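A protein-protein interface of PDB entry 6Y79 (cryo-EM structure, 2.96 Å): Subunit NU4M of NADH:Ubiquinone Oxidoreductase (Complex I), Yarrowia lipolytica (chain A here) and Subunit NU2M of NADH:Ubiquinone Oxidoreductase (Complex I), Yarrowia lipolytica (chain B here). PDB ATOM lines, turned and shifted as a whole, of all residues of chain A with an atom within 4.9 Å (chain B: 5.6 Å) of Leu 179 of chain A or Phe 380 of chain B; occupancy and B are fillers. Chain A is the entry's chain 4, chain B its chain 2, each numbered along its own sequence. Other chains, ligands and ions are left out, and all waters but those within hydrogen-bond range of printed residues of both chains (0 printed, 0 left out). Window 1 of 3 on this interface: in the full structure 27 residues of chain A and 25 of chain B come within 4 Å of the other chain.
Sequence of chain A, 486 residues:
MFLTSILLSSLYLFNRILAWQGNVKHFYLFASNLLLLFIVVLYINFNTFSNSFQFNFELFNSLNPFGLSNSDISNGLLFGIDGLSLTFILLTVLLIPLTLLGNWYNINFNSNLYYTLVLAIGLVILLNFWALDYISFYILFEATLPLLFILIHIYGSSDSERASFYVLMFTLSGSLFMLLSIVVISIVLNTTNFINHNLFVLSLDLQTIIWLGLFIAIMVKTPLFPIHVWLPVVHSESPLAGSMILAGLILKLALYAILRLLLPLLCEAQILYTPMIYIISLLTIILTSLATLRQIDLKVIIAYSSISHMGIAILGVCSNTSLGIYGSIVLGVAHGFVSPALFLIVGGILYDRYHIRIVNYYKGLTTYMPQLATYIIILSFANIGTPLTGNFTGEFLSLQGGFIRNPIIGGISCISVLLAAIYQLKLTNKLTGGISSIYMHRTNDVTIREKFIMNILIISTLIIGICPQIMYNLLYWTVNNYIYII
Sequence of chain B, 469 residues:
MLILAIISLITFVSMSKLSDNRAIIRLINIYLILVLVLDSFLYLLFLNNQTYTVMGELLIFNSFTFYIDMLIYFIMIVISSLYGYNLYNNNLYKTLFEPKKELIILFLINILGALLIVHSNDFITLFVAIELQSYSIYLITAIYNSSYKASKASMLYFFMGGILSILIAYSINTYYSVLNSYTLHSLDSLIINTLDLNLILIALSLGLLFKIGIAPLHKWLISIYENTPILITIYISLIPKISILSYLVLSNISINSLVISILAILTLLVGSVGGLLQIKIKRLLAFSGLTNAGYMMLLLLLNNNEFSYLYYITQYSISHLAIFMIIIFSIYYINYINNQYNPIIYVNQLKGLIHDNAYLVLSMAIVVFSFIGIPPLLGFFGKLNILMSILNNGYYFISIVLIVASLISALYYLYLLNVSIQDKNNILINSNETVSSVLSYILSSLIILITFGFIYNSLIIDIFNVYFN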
ATOM      1  N   ILE A 135       5.513 -27.098 -18.109  1.00  0.00           N
ATOM      2  CA  ILE A 135       4.146 -26.629 -18.291  1.00  0.00           C
ATOM      3  C   ILE A 135       4.009 -25.179 -17.836  1.00  0.00           C
ATOM      4  O   ILE A 135       3.239 -24.412 -18.420  1.00  0.00           O
ATOM      5  CB  ILE A 135       3.151 -27.583 -17.590  1.00  0.00           C
ATOM      6  CG1 ILE A 135       1.713 -27.283 -18.005  1.00  0.00           C
ATOM      7  CG2 ILE A 135       3.303 -27.582 -16.082  1.00  0.00           C
ATOM      8  CD1 ILE A 135       1.425 -27.643 -19.439  1.00  0.00           C
ATOM      9  N   TYR A 138       5.361 -23.303 -20.690  1.00  0.00           N
ATOM     10  CA  TYR A 138       4.509 -23.400 -21.865  1.00  0.00           C
ATOM     11  C   TYR A 138       3.246 -22.564 -21.725  1.00  0.00           C
ATOM     12  O   TYR A 138       2.713 -22.084 -22.729  1.00  0.00           O
ATOM     13  CB  TYR A 138       4.159 -24.858 -22.115  1.00  0.00           C
ATOM     14  CG  TYR A 138       3.422 -25.083 -23.397  1.00  0.00           C
ATOM     15  CD1 TYR A 138       4.105 -25.256 -24.584  1.00  0.00           C
ATOM     16  CD2 TYR A 138       2.038 -25.123 -23.425  1.00  0.00           C
ATOM     17  CE1 TYR A 138       3.432 -25.458 -25.748  1.00  0.00           C
ATOM     18  CE2 TYR A 138       1.377 -25.294 -24.582  1.00  0.00           C
ATOM     19  CZ  TYR A 138       2.068 -25.502 -25.724  1.00  0.00           C
ATOM     20  OH  TYR A 138       1.364 -25.678 -26.882  1.00  0.00           O
ATOM     21  N   ILE A 139       2.724 -22.417 -20.504  1.00  0.00           N
ATOM     22  CA  ILE A 139       1.491 -21.659 -20.312  1.00  0.00           C
ATOM     23  C   ILE A 139       1.715 -20.186 -20.623  1.00  0.00           C
ATOM     24  O   ILE A 139       0.962 -19.572 -21.387  1.00  0.00           O
ATOM     25  CB  ILE A 139       0.938 -21.866 -18.892  1.00  0.00           C
ATOM     26  CG1 ILE A 139       0.238 -23.211 -18.796  1.00  0.00           C
ATOM     27  CG2 ILE A 139      -0.062 -20.792 -18.532  1.00  0.00           C
ATOM     28  CD1 ILE A 139       0.039 -23.665 -17.384  1.00  0.00           C
ATOM     29  N   SER A 175       3.894 -24.597 -32.027  1.00  0.00           N
ATOM     30  CA  SER A 175       3.885 -24.760 -30.592  1.00  0.00           C
ATOM     31  C   SER A 175       2.966 -25.896 -30.140  1.00  0.00           C
ATOM     32  O   SER A 175       3.116 -26.398 -29.021  1.00  0.00           O
ATOM     33  CB  SER A 175       3.505 -23.430 -29.994  1.00  0.00           C
ATOM     34  OG  SER A 175       2.122 -23.203 -30.171  1.00  0.00           O
ATOM     35  N   LEU A 176       2.054 -26.357 -30.997  1.00  0.00           N
ATOM     36  CA  LEU A 176       1.305 -27.570 -30.675  1.00  0.00           C
ATOM     37  C   LEU A 176       2.200 -28.809 -30.689  1.00  0.00           C
ATOM     38  O   LEU A 176       2.069 -29.688 -29.828  1.00  0.00           O
ATOM     39  CB  LEU A 176       0.127 -27.733 -31.632  1.00  0.00           C
ATOM     40  CG  LEU A 176      -1.141 -26.952 -31.267  1.00  0.00           C
ATOM     41  CD1 LEU A 176      -2.325 -27.484 -32.023  1.00  0.00           C
ATOM     42  CD2 LEU A 176      -1.433 -26.978 -29.781  1.00  0.00           C
ATOM     43  N   PHE A 177       3.134 -28.897 -31.642  1.00  0.00           N
ATOM     44  CA  PHE A 177       4.096 -30.001 -31.631  1.00  0.00           C
ATOM     45  C   PHE A 177       5.054 -29.903 -30.450  1.00  0.00           C
ATOM     46  O   PHE A 177       5.486 -30.938 -29.902  1.00  0.00           O
ATOM     47  CB  PHE A 177       4.865 -30.038 -32.950  1.00  0.00           C
ATOM     48  CG  PHE A 177       4.021 -30.438 -34.119  1.00  0.00           C
ATOM     49  CD1 PHE A 177       3.733 -31.767 -34.359  1.00  0.00           C
ATOM     50  CD2 PHE A 177       3.494 -29.485 -34.964  1.00  0.00           C
ATOM     51  CE1 PHE A 177       2.939 -32.132 -35.422  1.00  0.00           C
ATOM     52  CE2 PHE A 177       2.704 -29.842 -36.027  1.00  0.00           C
ATOM     53  CZ  PHE A 177       2.426 -31.167 -36.256  1.00  0.00           C
ATOM     54  N   MET A 178       5.375 -28.670 -30.039  1.00  0.00           N
ATOM     55  CA  MET A 178       6.050 -28.475 -28.752  1.00  0.00           C
ATOM     56  C   MET A 178       5.260 -29.082 -27.599  1.00  0.00           C
ATOM     57  O   MET A 178       5.836 -29.730 -26.716  1.00  0.00           O
ATOM     58  CB  MET A 178       6.274 -26.993 -28.488  1.00  0.00           C
ATOM     59  CG  MET A 178       6.935 -26.672 -27.172  1.00  0.00           C
ATOM     60  SD  MET A 178       7.639 -25.022 -27.193  1.00  0.00           S
ATOM     61  CE  MET A 178       7.921 -24.752 -25.457  1.00  0.00           C
ATOM     62  N   LEU A 179       3.938 -28.896 -27.603  1.00  0.00           N
ATOM     63  CA  LEU A 179       3.105 -29.480 -26.555  1.00  0.00           C
ATOM     64  C   LEU A 179       3.108 -31.002 -26.610  1.00  0.00           C
ATOM     65  O   LEU A 179       3.044 -31.658 -25.568  1.00  0.00           O
ATOM     66  CB  LEU A 179       1.678 -28.951 -26.657  1.00  0.00           C
ATOM     67  CG  LEU A 179       0.730 -29.417 -25.562  1.00  0.00           C
ATOM     68  CD1 LEU A 179       1.169 -28.854 -24.234  1.00  0.00           C
ATOM     69  CD2 LEU A 179      -0.685 -29.048 -25.883  1.00  0.00           C
ATOM     70  N   LEU A 180       3.186 -31.578 -27.814  1.00  0.00           N
ATOM     71  CA  LEU A 180       3.301 -33.037 -27.959  1.00  0.00           C
ATOM     72  C   LEU A 180       4.522 -33.577 -27.239  1.00  0.00           C
ATOM     73  O   LEU A 180       4.432 -34.532 -26.455  1.00  0.00           O
ATOM     74  CB  LEU A 180       3.399 -33.443 -29.424  1.00  0.00           C
ATOM     75  CG  LEU A 180       2.175 -33.983 -30.127  1.00  0.00           C
ATOM     76  CD1 LEU A 180       1.338 -32.828 -30.292  1.00  0.00           C
ATOM     77  CD2 LEU A 180       2.539 -34.543 -31.475  1.00  0.00           C
ATOM     78  N   SER A 181       5.675 -32.957 -27.485  1.00  0.00           N
ATOM     79  CA  SER A 181       6.899 -33.409 -26.826  1.00  0.00           C
ATOM     80  C   SER A 181       6.882 -33.137 -25.326  1.00  0.00           C
ATOM     81  O   SER A 181       7.427 -33.927 -24.548  1.00  0.00           O
ATOM     82  CB  SER A 181       8.102 -32.757 -27.477  1.00  0.00           C
ATOM     83  OG  SER A 181       8.075 -33.053 -28.851  1.00  0.00           O
ATOM     84  N   ILE A 182       6.242 -32.044 -24.898  1.00  0.00           N
ATOM     85  CA  ILE A 182       6.129 -31.749 -23.469  1.00  0.00           C
ATOM     86  C   ILE A 182       5.248 -32.781 -22.767  1.00  0.00           C
ATOM     87  O   ILE A 182       5.542 -33.210 -21.644  1.00  0.00           O
ATOM     88  CB  ILE A 182       5.623 -30.304 -23.269  1.00  0.00           C
ATOM     89  CG1 ILE A 182       6.744 -29.313 -23.562  1.00  0.00           C
ATOM     90  CG2 ILE A 182       5.110 -30.053 -21.868  1.00  0.00           C
ATOM     91  CD1 ILE A 182       6.330 -27.885 -23.469  1.00  0.00           C
ATOM     92  N   VAL A 183       4.191 -33.242 -23.442  1.00  0.00           N
ATOM     93  CA  VAL A 183       3.326 -34.284 -22.886  1.00  0.00           C
ATOM     94  C   VAL A 183       4.072 -35.611 -22.781  1.00  0.00           C
ATOM     95  O   VAL A 183       3.946 -36.328 -21.779  1.00  0.00           O
ATOM     96  CB  VAL A 183       2.047 -34.410 -23.733  1.00  0.00           C
ATOM     97  CG1 VAL A 183       1.281 -35.659 -23.401  1.00  0.00           C
ATOM     98  CG2 VAL A 183       1.161 -33.248 -23.488  1.00  0.00           C
ATOM     99  N   SER B 370     -10.563 -20.174 -25.524  1.00  0.00           N
ATOM    100  CA  SER B 370     -10.640 -21.436 -24.790  1.00  0.00           C
ATOM    101  C   SER B 370     -11.128 -22.584 -25.660  1.00  0.00           C
ATOM    102  O   SER B 370     -10.783 -23.738 -25.395  1.00  0.00           O
ATOM    103  CB  SER B 370     -11.553 -21.292 -23.581  1.00  0.00           C
ATOM    104  OG  SER B 370     -11.572 -22.487 -22.831  1.00  0.00           O
ATOM    105  N   GLY B 373      -8.020 -23.652 -27.309  1.00  0.00           N
ATOM    106  CA  GLY B 373      -7.065 -24.279 -26.422  1.00  0.00           C
ATOM    107  C   GLY B 373      -5.844 -23.435 -26.140  1.00  0.00           C
ATOM    108  O   GLY B 373      -4.714 -23.876 -26.350  1.00  0.00           O
ATOM    109  N   ILE B 374      -6.063 -22.218 -25.672  1.00  0.00           N
ATOM    110  CA  ILE B 374      -4.990 -21.286 -25.328  1.00  0.00           C
ATOM    111  C   ILE B 374      -4.691 -21.428 -23.839  1.00  0.00           C
ATOM    112  O   ILE B 374      -5.630 -21.441 -23.036  1.00  0.00           O
ATOM    113  CB  ILE B 374      -5.379 -19.840 -25.690  1.00  0.00           C
ATOM    114  CG1 ILE B 374      -5.543 -19.703 -27.201  1.00  0.00           C
ATOM    115  CG2 ILE B 374      -4.363 -18.857 -25.217  1.00  0.00           C
ATOM    116  CD1 ILE B 374      -4.333 -20.082 -27.976  1.00  0.00           C
ATOM    117  N   PRO B 375      -3.419 -21.528 -23.441  1.00  0.00           N
ATOM    118  CA  PRO B 375      -3.041 -22.074 -22.125  1.00  0.00           C
ATOM    119  C   PRO B 375      -3.531 -21.351 -20.876  1.00  0.00           C
ATOM    120  O   PRO B 375      -3.699 -22.031 -19.852  1.00  0.00           O
ATOM    121  CB  PRO B 375      -1.520 -22.064 -22.202  1.00  0.00           C
ATOM    122  CG  PRO B 375      -1.269 -22.409 -23.558  1.00  0.00           C
ATOM    123  CD  PRO B 375      -2.275 -21.648 -24.358  1.00  0.00           C
ATOM    124  N   PRO B 376      -3.755 -20.030 -20.841  1.00  0.00           N
ATOM    125  CA  PRO B 376      -4.328 -19.476 -19.601  1.00  0.00           C
ATOM    126  C   PRO B 376      -5.772 -19.864 -19.343  1.00  0.00           C
ATOM    127  O   PRO B 376      -6.275 -19.595 -18.249  1.00  0.00           O
ATOM    128  CB  PRO B 376      -4.227 -17.966 -19.811  1.00  0.00           C
ATOM    129  CG  PRO B 376      -3.157 -17.810 -20.707  1.00  0.00           C
ATOM    130  CD  PRO B 376      -3.246 -18.919 -21.665  1.00  0.00           C
ATOM    131  N   LEU B 377      -6.451 -20.476 -20.299  1.00  0.00           N
ATOM    132  CA  LEU B 377      -7.871 -20.740 -20.224  1.00  0.00           C
ATOM    133  C   LEU B 377      -8.105 -22.226 -20.036  1.00  0.00           C
ATOM    134  O   LEU B 377      -7.186 -23.040 -20.102  1.00  0.00           O
ATOM    135  CB  LEU B 377      -8.571 -20.227 -21.480  1.00  0.00           C
ATOM    136  CG  LEU B 377      -8.256 -18.762 -21.751  1.00  0.00           C
ATOM    137  CD1 LEU B 377      -8.707 -18.384 -23.121  1.00  0.00           C
ATOM    138  CD2 LEU B 377      -8.911 -17.890 -20.734  1.00  0.00           C
ATOM    139  N   LEU B 378      -9.366 -22.567 -19.824  1.00  0.00           N
ATOM    140  CA  LEU B 378      -9.735 -23.876 -19.317  1.00  0.00           C
ATOM    141  C   LEU B 378      -9.799 -24.937 -20.403  1.00  0.00           C
ATOM    142  O   LEU B 378      -9.708 -26.125 -20.092  1.00  0.00           O
ATOM    143  CB  LEU B 378     -11.075 -23.745 -18.603  1.00  0.00           C
ATOM    144  CG  LEU B 378     -11.475 -24.707 -17.508  1.00  0.00           C
ATOM    145  CD1 LEU B 378     -12.133 -23.939 -16.429  1.00  0.00           C
ATOM    146  CD2 LEU B 378     -12.467 -25.627 -18.059  1.00  0.00           C
ATOM    147  N   GLY B 379      -9.938 -24.542 -21.667  1.00  0.00           N
ATOM    148  CA  GLY B 379     -10.007 -25.515 -22.744  1.00  0.00           C
ATOM    149  C   GLY B 379      -8.673 -26.135 -23.065  1.00  0.00           C
ATOM    150  O   GLY B 379      -8.605 -27.253 -23.599  1.00  0.00           O
ATOM    151  N   PHE B 380      -7.600 -25.433 -22.717  1.00  0.00           N
ATOM    152  CA  PHE B 380      -6.265 -25.947 -22.948  1.00  0.00           C
ATOM    153  C   PHE B 380      -5.982 -27.171 -22.104  1.00  0.00           C
ATOM    154  O   PHE B 380      -5.397 -28.136 -22.590  1.00  0.00           O
ATOM    155  CB  PHE B 380      -5.223 -24.901 -22.636  1.00  0.00           C
ATOM    156  CG  PHE B 380      -3.851 -25.429 -22.771  1.00  0.00           C
ATOM    157  CD1 PHE B 380      -3.389 -25.787 -24.019  1.00  0.00           C
ATOM    158  CD2 PHE B 380      -3.048 -25.645 -21.666  1.00  0.00           C
ATOM    159  CE1 PHE B 380      -2.158 -26.306 -24.165  1.00  0.00           C
ATOM    160  CE2 PHE B 380      -1.810 -26.172 -21.811  1.00  0.00           C
ATOM    161  CZ  PHE B 380      -1.369 -26.508 -23.053  1.00  0.00           C
ATOM    162  N   PHE B 381      -6.336 -27.126 -20.823  1.00  0.00           N
ATOM    163  CA  PHE B 381      -6.077 -28.262 -19.956  1.00  0.00           C
ATOM    164  C   PHE B 381      -6.963 -29.444 -20.293  1.00  0.00           C
ATOM    165  O   PHE B 381      -6.549 -30.583 -20.070  1.00  0.00           O
ATOM    166  CB  PHE B 381      -6.250 -27.856 -18.501  1.00  0.00           C
ATOM    167  CG  PHE B 381      -5.217 -26.895 -18.031  1.00  0.00           C
ATOM    168  CD1 PHE B 381      -3.969 -27.342 -17.644  1.00  0.00           C
ATOM    169  CD2 PHE B 381      -5.483 -25.542 -17.993  1.00  0.00           C
ATOM    170  CE1 PHE B 381      -3.010 -26.457 -17.223  1.00  0.00           C
ATOM    171  CE2 PHE B 381      -4.527 -24.655 -17.577  1.00  0.00           C
ATOM    172  CZ  PHE B 381      -3.294 -25.111 -17.185  1.00  0.00           C
ATOM    173  N   GLY B 382      -8.135 -29.201 -20.877  1.00  0.00           N
ATOM    174  CA  GLY B 382      -8.928 -30.293 -21.409  1.00  0.00           C
ATOM    175  C   GLY B 382      -8.243 -30.993 -22.564  1.00  0.00           C
ATOM    176  O   GLY B 382      -8.109 -32.221 -22.566  1.00  0.00           O
ATOM    177  N   LYS B 383      -7.776 -30.218 -23.551  1.00  0.00           N
ATOM    178  CA  LYS B 383      -7.056 -30.817 -24.675  1.00  0.00           C
ATOM    179  C   LYS B 383      -5.734 -31.439 -24.239  1.00  0.00           C
ATOM    180  O   LYS B 383      -5.325 -32.478 -24.772  1.00  0.00           O
ATOM    181  CB  LYS B 383      -6.825 -29.771 -25.762  1.00  0.00           C
ATOM    182  CG  LYS B 383      -8.107 -29.279 -26.389  1.00  0.00           C
ATOM    183  CD  LYS B 383      -7.867 -28.420 -27.608  1.00  0.00           C
ATOM    184  CE  LYS B 383      -9.186 -28.027 -28.229  1.00  0.00           C
ATOM    185  NZ  LYS B 383     -10.130 -27.517 -27.193  1.00  0.00           N
ATOM    186  N   LEU B 384      -5.095 -30.853 -23.229  1.00  0.00           N
ATOM    187  CA  LEU B 384      -3.840 -31.363 -22.697  1.00  0.00           C
ATOM    188  C   LEU B 384      -4.028 -32.709 -22.016  1.00  0.00           C
ATOM    189  O   LEU B 384      -3.254 -33.643 -22.242  1.00  0.00           O
ATOM    190  CB  LEU B 384      -3.271 -30.350 -21.712  1.00  0.00           C
ATOM    191  CG  LEU B 384      -2.060 -30.765 -20.899  1.00  0.00           C
ATOM    192  CD1 LEU B 384      -0.882 -30.746 -21.786  1.00  0.00           C
ATOM    193  CD2 LEU B 384      -1.859 -29.819 -19.756  1.00  0.00           C
ATOM    194  N   ASN B 385      -5.049 -32.827 -21.173  1.00  0.00           N
ATOM    195  CA  ASN B 385      -5.297 -34.085 -20.494  1.00  0.00           C
ATOM    196  C   ASN B 385      -5.885 -35.139 -21.413  1.00  0.00           C
ATOM    197  O   ASN B 385      -5.789 -36.326 -21.102  1.00  0.00           O
ATOM    198  CB  ASN B 385      -6.207 -33.851 -19.294  1.00  0.00           C
ATOM    199  CG  ASN B 385      -5.528 -33.046 -18.216  1.00  0.00           C
ATOM    200  OD1 ASN B 385      -4.423 -33.368 -17.791  1.00  0.00           O
ATOM    201  ND2 ASN B 385      -6.174 -31.976 -17.784  1.00  0.00           N
ATOM    202  N   LEU B 387      -4.621 -35.368 -24.544  1.00  0.00           N
ATOM    203  CA  LEU B 387      -3.360 -35.785 -25.163  1.00  0.00           C
ATOM    204  C   LEU B 387      -2.536 -36.678 -24.245  1.00  0.00           C
ATOM    205  O   LEU B 387      -1.873 -37.608 -24.711  1.00  0.00           O
ATOM    206  CB  LEU B 387      -2.534 -34.563 -25.545  1.00  0.00           C
ATOM    207  CG  LEU B 387      -2.903 -33.758 -26.778  1.00  0.00           C
ATOM    208  CD1 LEU B 387      -2.085 -32.483 -26.787  1.00  0.00           C
ATOM    209  CD2 LEU B 387      -2.647 -34.573 -28.017  1.00  0.00           C
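Leu 179 of chain A touches just these residues of chain B: Phe 380 (3.6 Å), Leu 384 (3.7 Å) and Leu 387 (3.8 Å). Phe 380 of chain B touches just these residues of chain A: Tyr 138 (3.4 Å) and Leu 179 (3.6 Å). Printed residues of chain B within 4 Å of Val 183 of chain A: Leu 384 and Leu 387. Printed residues of chain B within 4 Å of Ile 135 of chain A: Leu 384 (3.95 Å). Printed residues of chain A within 4 Å of Leu 384 of chain B: Ile 135 (3.95 Å), Leu 179 (3.7 Å) and Val 183 (3.7 Å). Printed residues of chain A within 4 Å of Pro 375 of chain B: Ile 139. Of the printed residues of chain A, Leu 387 of chain B touches Leu 179 and Val 183. Asn 385 of chain B touches none of the printed residues of chain A. Lys 383 of chain B touches none of the printed residues of chain A. The nearest printed residue of chain B that does not touch Leu 179 of chain A is Lys 383 of chain B (5.8 Å). The nearest printed residue of chain B that does not touch Ile 135 of chain A is Phe 380 of chain B (4.3 Å).
Hydrophobic or aromatic side chains of chain B that line the printed part of chain A: Pro 375, Phe 380, Phe 381, Leu 384 and Leu 387. Hydrophobic or aromatic side chains of chain A within 4 Å of the printed part of chain B: Ile 135, Tyr 138, Ile 139, Leu 179 and Val 183. Among the printed residues, 9 pairs touch across the chains.
Among the printed residues, pairs that only touch across the chains: Ile 135 of chain A with Leu 384 of chain B (3.95 Å), Tyr 138 of chain A with Phe 380 of chain B (3.4 Å), Ile 139 of chain A with Pro 375 of chain B (3.6 Å), Ile 139 of chain A with Phe 381 of chain B (3.6 Å), Leu 179 of chain A with Phe 380 of chain B (3.6 Å), Leu 179 of chain A with Leu 384 of chain B (3.7 Å), Leu 179 of chain A with Leu 387 of chain B (3.8 Å), Val 183 of chain A with Leu 384 of chain B (3.7 Å) and Val 183 of chain A with Leu 387 of chain B (3.9 Å).
The backbone carbonyl oxygen of Phe 381 of chain B is in hydrogen-bond range of the side-chain amide nitrogen of Asn 385 of chain B (2.7 Å). O of Ser 175 of chain A is in hydrogen-bond range of OH of Tyr 138 of chain A (2.9 Å).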
